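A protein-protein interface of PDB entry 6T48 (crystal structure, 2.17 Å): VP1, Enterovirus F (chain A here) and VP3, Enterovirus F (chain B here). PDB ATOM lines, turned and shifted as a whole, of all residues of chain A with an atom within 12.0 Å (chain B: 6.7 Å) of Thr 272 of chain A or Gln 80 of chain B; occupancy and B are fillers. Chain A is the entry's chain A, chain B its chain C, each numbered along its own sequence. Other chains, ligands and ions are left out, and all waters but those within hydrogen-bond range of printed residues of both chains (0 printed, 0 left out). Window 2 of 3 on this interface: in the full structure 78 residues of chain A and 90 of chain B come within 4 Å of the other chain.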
ATOM      1  N   ASN A 267      -6.543  15.001 -23.646  1.00  0.00           N
ATOM      2  CA  ASN A 267      -5.971  16.195 -24.255  1.00  0.00           C
ATOM      3  C   ASN A 267      -6.047  17.418 -23.354  1.00  0.00           C
ATOM      4  O   ASN A 267      -6.810  17.453 -22.389  1.00  0.00           O
ATOM      5  CB  ASN A 267      -6.691  16.531 -25.564  1.00  0.00           C
ATOM      6  CG  ASN A 267      -6.487  15.482 -26.631  1.00  0.00           C
ATOM      7  OD1 ASN A 267      -5.388  14.955 -26.796  1.00  0.00           O
ATOM      8  ND2 ASN A 267      -7.546  15.183 -27.375  1.00  0.00           N
ATOM      9  N   ARG A 268      -5.236  18.417 -23.684  1.00  0.00           N
ATOM     10  CA  ARG A 268      -5.222  19.683 -22.969  1.00  0.00           C
ATOM     11  C   ARG A 268      -5.321  20.752 -24.050  1.00  0.00           C
ATOM     12  O   ARG A 268      -5.163  20.454 -25.237  1.00  0.00           O
ATOM     13  CB  ARG A 268      -3.935  19.859 -22.157  1.00  0.00           C
ATOM     14  CG  ARG A 268      -2.657  19.689 -22.946  1.00  0.00           C
ATOM     15  CD  ARG A 268      -1.460  20.125 -22.116  1.00  0.00           C
ATOM     16  NE  ARG A 268      -0.215  19.537 -22.602  1.00  0.00           N
ATOM     17  CZ  ARG A 268       0.996  19.984 -22.287  1.00  0.00           C
ATOM     18  NH1 ARG A 268       2.071  19.379 -22.772  1.00  0.00           N
ATOM     19  NH2 ARG A 268       1.133  21.045 -21.501  1.00  0.00           N
ATOM     20  N   ALA A 269      -5.583  21.990 -23.648  1.00  0.00           N
ATOM     21  CA  ALA A 269      -5.733  23.084 -24.601  1.00  0.00           C
ATOM     22  C   ALA A 269      -4.524  23.298 -25.504  1.00  0.00           C
ATOM     23  O   ALA A 269      -4.662  23.362 -26.725  1.00  0.00           O
ATOM     24  CB  ALA A 269      -6.060  24.375 -23.859  1.00  0.00           C
ATOM     25  N   ARG A 270      -3.342  23.412 -24.907  1.00  0.00           N
ATOM     26  CA  ARG A 270      -2.133  23.644 -25.689  1.00  0.00           C
ATOM     27  C   ARG A 270      -0.886  23.093 -25.011  1.00  0.00           C
ATOM     28  O   ARG A 270      -0.822  22.996 -23.785  1.00  0.00           O
ATOM     29  CB  ARG A 270      -1.973  25.142 -25.951  1.00  0.00           C
ATOM     30  CG  ARG A 270      -1.833  25.982 -24.697  1.00  0.00           C
ATOM     31  CD  ARG A 270      -2.124  27.448 -25.000  1.00  0.00           C
ATOM     32  NE  ARG A 270      -3.552  27.691 -25.186  1.00  0.00           N
ATOM     33  CZ  ARG A 270      -4.438  27.759 -24.193  1.00  0.00           C
ATOM     34  NH1 ARG A 270      -4.047  27.608 -22.931  1.00  0.00           N
ATOM     35  NH2 ARG A 270      -5.719  27.972 -24.463  1.00  0.00           N
ATOM     36  N   ILE A 271       0.104  22.743 -25.826  1.00  0.00           N
ATOM     37  CA  ILE A 271       1.354  22.166 -25.345  1.00  0.00           C
ATOM     38  C   ILE A 271       2.168  23.109 -24.453  1.00  0.00           C
ATOM     39  O   ILE A 271       3.040  22.661 -23.709  1.00  0.00           O
ATOM     40  CB  ILE A 271       2.230  21.706 -26.542  1.00  0.00           C
ATOM     41  CG1 ILE A 271       3.311  20.736 -26.063  1.00  0.00           C
ATOM     42  CG2 ILE A 271       2.876  22.915 -27.220  1.00  0.00           C
ATOM     43  CD1 ILE A 271       4.134  20.137 -27.196  1.00  0.00           C
ATOM     44  N   THR A 272       1.871  24.405 -24.515  1.00  0.00           N
ATOM     45  CA  THR A 272       2.592  25.401 -23.721  1.00  0.00           C
ATOM     46  C   THR A 272       1.956  25.765 -22.380  1.00  0.00           C
ATOM     47  O   THR A 272       2.453  26.639 -21.672  1.00  0.00           O
ATOM     48  CB  THR A 272       2.795  26.701 -24.520  1.00  0.00           C
ATOM     49  OG1 THR A 272       1.549  27.102 -25.105  1.00  0.00           O
ATOM     50  CG2 THR A 272       3.831  26.492 -25.618  1.00  0.00           C
ATOM     51  N   THR A 273       0.857  25.105 -22.032  1.00  0.00           N
ATOM     52  CA  THR A 273       0.193  25.374 -20.760  1.00  0.00           C
ATOM     53  C   THR A 273       0.090  24.071 -19.980  1.00  0.00           C
ATOM     54  O   THR A 273      -0.661  23.172 -20.355  1.00  0.00           O
ATOM     55  CB  THR A 273      -1.220  25.957 -20.973  1.00  0.00           C
ATOM     56  OG1 THR A 273      -1.120  27.221 -21.639  1.00  0.00           O
ATOM     57  CG2 THR A 273      -1.921  26.152 -19.637  1.00  0.00           C
ATOM     58  N   ALA A 274       0.858  23.974 -18.900  1.00  0.00           N
ATOM     59  CA  ALA A 274       0.880  22.776 -18.067  1.00  0.00           C
ATOM     60  C   ALA A 274      -0.340  22.656 -17.160  1.00  0.00           C
ATOM     61  O   ALA A 274      -0.862  21.527 -17.035  1.00  0.00           O
ATOM     62  CB  ALA A 274       2.155  22.749 -17.232  1.00  0.00           C
ATOM     63  N   VAL B  58      -2.749  17.190 -27.590  1.00  0.00           N
ATOM     64  CA  VAL B  58      -3.747  18.183 -27.960  1.00  0.00           C
ATOM     65  C   VAL B  58      -4.686  17.598 -29.011  1.00  0.00           C
ATOM     66  O   VAL B  58      -4.366  16.603 -29.657  1.00  0.00           O
ATOM     67  CB  VAL B  58      -3.086  19.461 -28.519  1.00  0.00           C
ATOM     68  CG1 VAL B  58      -2.215  20.101 -27.451  1.00  0.00           C
ATOM     69  CG2 VAL B  58      -2.251  19.126 -29.739  1.00  0.00           C
ATOM     70  N   GLN B  74      11.233  30.903 -35.942  1.00  0.00           N
ATOM     71  CA  GLN B  74      10.534  32.028 -35.332  1.00  0.00           C
ATOM     72  C   GLN B  74      10.780  33.351 -36.054  1.00  0.00           C
ATOM     73  O   GLN B  74      11.719  33.476 -36.841  1.00  0.00           O
ATOM     74  CB  GLN B  74      10.990  32.178 -33.880  1.00  0.00           C
ATOM     75  CG  GLN B  74      10.805  30.926 -33.047  1.00  0.00           C
ATOM     76  CD  GLN B  74       9.349  30.641 -32.776  1.00  0.00           C
ATOM     77  OE1 GLN B  74       8.681  31.395 -32.069  1.00  0.00           O
ATOM     78  NE2 GLN B  74       8.842  29.552 -33.343  1.00  0.00           N
ATOM     79  N   MET B  77      11.434  36.804 -30.706  1.00  0.00           N
ATOM     80  CA  MET B  77      12.388  36.174 -29.804  1.00  0.00           C
ATOM     81  C   MET B  77      11.842  35.712 -28.461  1.00  0.00           C
ATOM     82  O   MET B  77      10.749  36.102 -28.049  1.00  0.00           O
ATOM     83  CB  MET B  77      13.573  37.118 -29.582  1.00  0.00           C
ATOM     84  CG  MET B  77      14.386  37.337 -30.851  1.00  0.00           C
ATOM     85  SD  MET B  77      15.650  38.604 -30.724  1.00  0.00           S
ATOM     86  CE  MET B  77      14.649  40.084 -30.698  1.00  0.00           C
ATOM     87  N   ASP B  78      12.614  34.842 -27.810  1.00  0.00           N
ATOM     88  CA  ASP B  78      12.313  34.311 -26.478  1.00  0.00           C
ATOM     89  C   ASP B  78      10.999  33.541 -26.307  1.00  0.00           C
ATOM     90  O   ASP B  78      10.514  33.386 -25.186  1.00  0.00           O
ATOM     91  CB  ASP B  78      12.364  35.460 -25.455  1.00  0.00           C
ATOM     92  CG  ASP B  78      13.510  36.446 -25.726  1.00  0.00           C
ATOM     93  OD1 ASP B  78      14.609  36.002 -26.119  1.00  0.00           O
ATOM     94  OD2 ASP B  78      13.316  37.666 -25.534  1.00  0.00           O
ATOM     95  N   GLY B  79      10.439  33.045 -27.406  1.00  0.00           N
ATOM     96  CA  GLY B  79       9.177  32.322 -27.336  1.00  0.00           C
ATOM     97  C   GLY B  79       9.205  30.974 -26.632  1.00  0.00           C
ATOM     98  O   GLY B  79      10.249  30.336 -26.530  1.00  0.00           O
ATOM     99  N   GLN B  80       8.044  30.537 -26.152  1.00  0.00           N
ATOM    100  CA  GLN B  80       7.932  29.262 -25.454  1.00  0.00           C
ATOM    101  C   GLN B  80       7.656  28.111 -26.418  1.00  0.00           C
ATOM    102  O   GLN B  80       6.998  28.286 -27.445  1.00  0.00           O
ATOM    103  CB  GLN B  80       6.824  29.337 -24.400  1.00  0.00           C
ATOM    104  CG  GLN B  80       6.675  28.070 -23.570  1.00  0.00           C
ATOM    105  CD  GLN B  80       5.680  28.226 -22.433  1.00  0.00           C
ATOM    106  OE1 GLN B  80       4.831  29.117 -22.450  1.00  0.00           O
ATOM    107  NE2 GLN B  80       5.772  27.348 -21.443  1.00  0.00           N
ATOM    108  N   ILE B  81       8.162  26.931 -26.073  1.00  0.00           N
ATOM    109  CA  ILE B  81       7.997  25.743 -26.900  1.00  0.00           C
ATOM    110  C   ILE B  81       7.062  24.715 -26.255  1.00  0.00           C
ATOM    111  O   ILE B  81       6.217  24.132 -26.932  1.00  0.00           O
ATOM    112  CB  ILE B  81       9.370  25.104 -27.179  1.00  0.00           C
ATOM    113  CG1 ILE B  81      10.230  26.089 -27.973  1.00  0.00           C
ATOM    114  CG2 ILE B  81       9.202  23.798 -27.933  1.00  0.00           C
ATOM    115  CD1 ILE B  81      11.693  25.707 -28.045  1.00  0.00           C
ATOM    116  N   MET B  82       7.215  24.485 -24.954  1.00  0.00           N
ATOM    117  CA  MET B  82       6.348  23.540 -24.252  1.00  0.00           C
ATOM    118  C   MET B  82       6.384  23.747 -22.744  1.00  0.00           C
ATOM    119  O   MET B  82       7.226  24.488 -22.232  1.00  0.00           O
ATOM    120  CB  MET B  82       6.715  22.084 -24.601  1.00  0.00           C
ATOM    121  CG  MET B  82       8.086  21.589 -24.149  1.00  0.00           C
ATOM    122  SD  MET B  82       8.252  21.218 -22.377  1.00  0.00           S
ATOM    123  CE  MET B  82       7.226  19.863 -22.195  1.00  0.00           C
ATOM    124  N   ALA B  83       5.449  23.106 -22.049  1.00  0.00           N
ATOM    125  CA  ALA B  83       5.351  23.183 -20.592  1.00  0.00           C
ATOM    126  C   ALA B  83       4.760  21.872 -20.089  1.00  0.00           C
ATOM    127  O   ALA B  83       4.007  21.215 -20.806  1.00  0.00           O
ATOM    128  CB  ALA B  83       4.458  24.350 -20.180  1.00  0.00           C
ATOM    129  N   LEU B  84       5.096  21.496 -18.859  1.00  0.00           N
ATOM    130  CA  LEU B  84       4.590  20.255 -18.280  1.00  0.00           C
ATOM    131  C   LEU B  84       4.847  20.184 -16.776  1.00  0.00           C
ATOM    132  O   LEU B  84       5.884  20.646 -16.306  1.00  0.00           O
ATOM    133  CB  LEU B  84       5.275  19.057 -18.951  1.00  0.00           C
ATOM    134  CG  LEU B  84       4.944  17.663 -18.410  1.00  0.00           C
ATOM    135  CD1 LEU B  84       3.567  17.241 -18.887  1.00  0.00           C
ATOM    136  CD2 LEU B  84       5.986  16.665 -18.879  1.00  0.00           C
ATOM    137  N   GLN B 140       3.368  28.128 -13.329  1.00  0.00           N
ATOM    138  CA  GLN B 140       4.450  27.916 -14.277  1.00  0.00           C
ATOM    139  C   GLN B 140       4.939  29.289 -14.725  1.00  0.00           C
ATOM    140  O   GLN B 140       4.164  30.244 -14.777  1.00  0.00           O
ATOM    141  CB  GLN B 140       3.968  27.109 -15.484  1.00  0.00           C
ATOM    142  CG  GLN B 140       3.091  27.880 -16.454  1.00  0.00           C
ATOM    143  CD  GLN B 140       2.796  27.092 -17.720  1.00  0.00           C
ATOM    144  OE1 GLN B 140       2.002  26.154 -17.708  1.00  0.00           O
ATOM    145  NE2 GLN B 140       3.449  27.464 -18.817  1.00  0.00           N
ATOM    146  N   PRO B 141       6.235  29.411 -15.041  1.00  0.00           N
ATOM    147  CA  PRO B 141       6.769  30.704 -15.478  1.00  0.00           C
ATOM    148  C   PRO B 141       6.075  31.201 -16.745  1.00  0.00           C
ATOM    149  O   PRO B 141       5.773  30.419 -17.649  1.00  0.00           O
ATOM    150  CB  PRO B 141       8.259  30.415 -15.674  1.00  0.00           C
ATOM    151  CG  PRO B 141       8.282  28.960 -16.020  1.00  0.00           C
ATOM    152  CD  PRO B 141       7.275  28.370 -15.068  1.00  0.00           C
ATOM    153  N   THR B 142       5.825  32.507 -16.794  1.00  0.00           N
ATOM    154  CA  THR B 142       5.135  33.139 -17.917  1.00  0.00           C
ATOM    155  C   THR B 142       6.033  33.515 -19.092  1.00  0.00           C
ATOM    156  O   THR B 142       5.571  33.586 -20.231  1.00  0.00           O
ATOM    157  CB  THR B 142       4.390  34.402 -17.445  1.00  0.00           C
ATOM    158  OG1 THR B 142       5.313  35.290 -16.799  1.00  0.00           O
ATOM    159  CG2 THR B 142       3.288  34.028 -16.464  1.00  0.00           C
ATOM    160  N   ASN B 143       7.308  33.771 -18.815  1.00  0.00           N
ATOM    161  CA  ASN B 143       8.252  34.127 -19.870  1.00  0.00           C
ATOM    162  C   ASN B 143       9.618  33.499 -19.615  1.00  0.00           C
ATOM    163  O   ASN B 143       9.877  32.968 -18.534  1.00  0.00           O
ATOM    164  CB  ASN B 143       8.377  35.652 -19.987  1.00  0.00           C
ATOM    165  CG  ASN B 143       8.769  36.313 -18.680  1.00  0.00           C
ATOM    166  OD1 ASN B 143       9.812  36.007 -18.103  1.00  0.00           O
ATOM    167  ND2 ASN B 143       7.933  37.230 -18.207  1.00  0.00           N
ATOM    168  N   ILE B 195       8.308  21.974 -15.802  1.00  0.00           N
ATOM    169  CA  ILE B 195       9.423  21.925 -16.725  1.00  0.00           C
ATOM    170  C   ILE B 195       8.917  22.692 -17.955  1.00  0.00           C
ATOM    171  O   ILE B 195       7.812  22.445 -18.439  1.00  0.00           O
ATOM    172  CB  ILE B 195       9.805  20.461 -17.075  1.00  0.00           C
ATOM    173  CG1 ILE B 195      11.002  20.449 -18.015  1.00  0.00           C
ATOM    174  CG2 ILE B 195       8.633  19.741 -17.704  1.00  0.00           C
ATOM    175  CD1 ILE B 195      11.559  19.066 -18.255  1.00  0.00           C
ATOM    176  N   THR B 196       9.693  23.666 -18.417  1.00  0.00           N
ATOM    177  CA  THR B 196       9.307  24.451 -19.585  1.00  0.00           C
ATOM    178  C   THR B 196      10.482  24.574 -20.545  1.00  0.00           C
ATOM    179  O   THR B 196      11.640  24.473 -20.139  1.00  0.00           O
ATOM    180  CB  THR B 196       8.825  25.872 -19.199  1.00  0.00           C
ATOM    181  OG1 THR B 196       9.874  26.571 -18.520  1.00  0.00           O
ATOM    182  CG2 THR B 196       7.601  25.797 -18.301  1.00  0.00           C
ATOM    183  N   MET B 197      10.176  24.786 -21.819  1.00  0.00           N
ATOM    184  CA  MET B 197      11.205  24.908 -22.841  1.00  0.00           C
ATOM    185  C   MET B 197      10.963  26.188 -23.625  1.00  0.00           C
ATOM    186  O   MET B 197       9.820  26.512 -23.947  1.00  0.00           O
ATOM    187  CB  MET B 197      11.151  23.702 -23.780  1.00  0.00           C
ATOM    188  CG  MET B 197      12.289  23.632 -24.782  1.00  0.00           C
ATOM    189  SD  MET B 197      12.106  22.232 -25.916  1.00  0.00           S
ATOM    190  CE  MET B 197      12.648  20.863 -24.874  1.00  0.00           C
ATOM    191  N   TRP B 198      12.039  26.905 -23.933  1.00  0.00           N
ATOM    192  CA  TRP B 198      11.945  28.167 -24.665  1.00  0.00           C
ATOM    193  C   TRP B 198      13.044  28.275 -25.711  1.00  0.00           C
ATOM    194  O   TRP B 198      14.081  27.622 -25.608  1.00  0.00           O
ATOM    195  CB  TRP B 198      12.088  29.355 -23.699  1.00  0.00           C
ATOM    196  CG  TRP B 198      11.283  29.226 -22.436  1.00  0.00           C
ATOM    197  CD1 TRP B 198      11.515  28.369 -21.392  1.00  0.00           C
ATOM    198  CD2 TRP B 198      10.079  29.931 -22.114  1.00  0.00           C
ATOM    199  NE1 TRP B 198      10.523  28.495 -20.445  1.00  0.00           N
ATOM    200  CE2 TRP B 198       9.629  29.445 -20.863  1.00  0.00           C
ATOM    201  CE3 TRP B 198       9.333  30.926 -22.762  1.00  0.00           C
ATOM    202  CZ2 TRP B 198       8.466  29.918 -20.251  1.00  0.00           C
ATOM    203  CZ3 TRP B 198       8.175  31.396 -22.151  1.00  0.00           C
ATOM    204  CH2 TRP B 198       7.754  30.889 -20.908  1.00  0.00           C
ATOM    205  N   TYR B 199      12.813  29.098 -26.726  1.00  0.00           N
ATOM    206  CA  TYR B 199      13.829  29.316 -27.744  1.00  0.00           C
ATOM    207  C   TYR B 199      14.903  30.159 -27.059  1.00  0.00           C
ATOM    208  O   TYR B 199      14.584  31.183 -26.448  1.00  0.00           O
ATOM    209  CB  TYR B 199      13.244  30.096 -28.930  1.00  0.00           C
ATOM    210  CG  TYR B 199      12.361  29.262 -29.833  1.00  0.00           C
ATOM    211  CD1 TYR B 199      12.915  28.435 -30.810  1.00  0.00           C
ATOM    212  CD2 TYR B 199      10.973  29.255 -29.672  1.00  0.00           C
ATOM    213  CE1 TYR B 199      12.108  27.614 -31.606  1.00  0.00           C
ATOM    214  CE2 TYR B 199      10.157  28.438 -30.460  1.00  0.00           C
ATOM    215  CZ  TYR B 199      10.734  27.619 -31.422  1.00  0.00           C
ATOM    216  OH  TYR B 199       9.942  26.785 -32.178  1.00  0.00           O
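Of the printed residues of chain B, Thr 272 of chain A touches Gln 80, Ile 81, Met 82, Ala 83 and Gln 140.
Gln 80 of chain B touches just one residue of chain A: Thr 272.
Ile 81 of chain B touches just these residues of chain A: Ile 271 (3.6 Å) and Thr 272 (3.6 Å).
Of chain A, only Arg 268, Ile 271, Thr 272 and Ala 274 come within 4 Å of Ala 83 of chain B.
No residue of chain A comes within 4 Å of Pro 141 of chain B.
No residue of chain A comes within 4 Å of Trp 198 of chain B.
Tyr 199 of chain B touches none of the printed residues of chain A.
Of the printed residues of chain B, Asn 267 of chain A touches Val 58.
Printed residues of chain A within 4 Å of Met 82 of chain B: Ile 271 (3.5 Å) and Thr 272 (3.99 Å).
Printed residues of chain A within 4 Å of Val 58 of chain B: Asn 267, Arg 268, Arg 270 and Ile 271.
Of the printed residues of chain B, Arg 270 of chain A touches Val 58.
Printed residues of chain A within 4 Å of Gln 140 of chain B: Thr 272, Thr 273 and Ala 274.
Asn 143 of chain B touches none of the printed residues of chain A.
The nearest printed residue of chain B that does not touch Thr 272 of chain A is Thr 196 of chain B (6.2 Å).
The nearest residue of chain A that does not touch Gln 80 of chain B is Thr 273 of chain A (5.4 Å).
The nearest printed residue of chain A that does not touch Met 82 of chain B is Arg 268 of chain A (5.2 Å).
Among the printed residues, pairs that only touch across the chains: Arg 268 of chain A with Val 58 of chain B (3.7 Å), Arg 270 of chain A with Val 58 of chain B (3.96 Å), Ile 271 of chain A with Val 58 of chain B (3.9 Å), Ile 271 of chain A with Ile 81 of chain B (3.6 Å), Ile 271 of chain A with Met 82 of chain B (3.5 Å), Thr 272 of chain A with Ile 81 of chain B (3.6 Å), Thr 272 of chain A with Met 82 of chain B (3.99 Å), Thr 272 of chain A with Ala 83 of chain B (3.4 Å), Thr 273 of chain A with Gln 140 of chain B (3.6 Å), Ala 274 of chain A with Ala 83 of chain B (3.8 Å) and Ala 274 of chain A with Leu 84 of chain B (3.6 Å).
Of the 8 printed residues of chain A, 7 touch a printed residue of chain B.
Printed residues of chain A that touch a printed residue of chain B: Asn 267, Arg 268, Arg 270, Ile 271, Thr 272, Thr 273 and Ala 274.
Hydrophobic or aromatic side chains of chain A within 4 Å of the printed part of chain B: Ile 271 and Ala 274.
Hydrophobic or aromatic side chains of chain B that line the printed part of chain A: Val 58, Met 82 and Ala 83.
Among the printed residues, no Asp or Glu carboxylate lies within 4 Å of a Lys or Arg side-chain nitrogen of the other chain.
The side-chain amide oxygen (OD1) of Asn 267 of chain A sits close to the backbone carbonyl oxygen (O) of Val 58 of chain B.
The guanidinium group of Arg 268 of chain A sits at hydrogen-bond distance from the backbone carbonyl oxygen of Ala 83 of chain B (3.0 Å).
The backbone carbonyl oxygen of Ile 271 of chain A is in hydrogen-bond range of the backbone NH of Ala 83 of chain B (3.0 Å).
O of Thr 272 of chain A is in hydrogen-bond range of NE2 of Gln 80 of chain B.
The backbone carbonyl oxygen (O) of Thr 272 of chain A lies within hydrogen-bond range of the side-chain amide nitrogen (NE2) of Gln 140 of chain B.
N of Ala 274 of chain A is in hydrogen-bond range of OE1 of Gln 140 of chain B (2.7 Å).
The backbone carbonyl oxygen of Ile 271 of chain A sits at hydrogen-bond distance from the guanidinium group of Arg 268 of chain A (3.3 Å).
The backbone carbonyl oxygen of Thr 273 of chain A is in hydrogen-bond range of the guanidinium group of Arg 268 of chain A.
O of Met 82 of chain B sits at hydrogen-bond distance from NE2 of Gln 80 of chain B, at 3.3 Å.
The backbone NH of Ile 81 of chain B is in hydrogen-bond range of the backbone carbonyl oxygen of Met 197 of chain B (2.7 Å).
O of Met 82 of chain B sits at hydrogen-bond distance from N of Met 197 of chain B (3.0 Å).
The backbone NH of Ile 195 of chain B is in hydrogen-bond range of the backbone carbonyl oxygen of Leu 84 of chain B.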
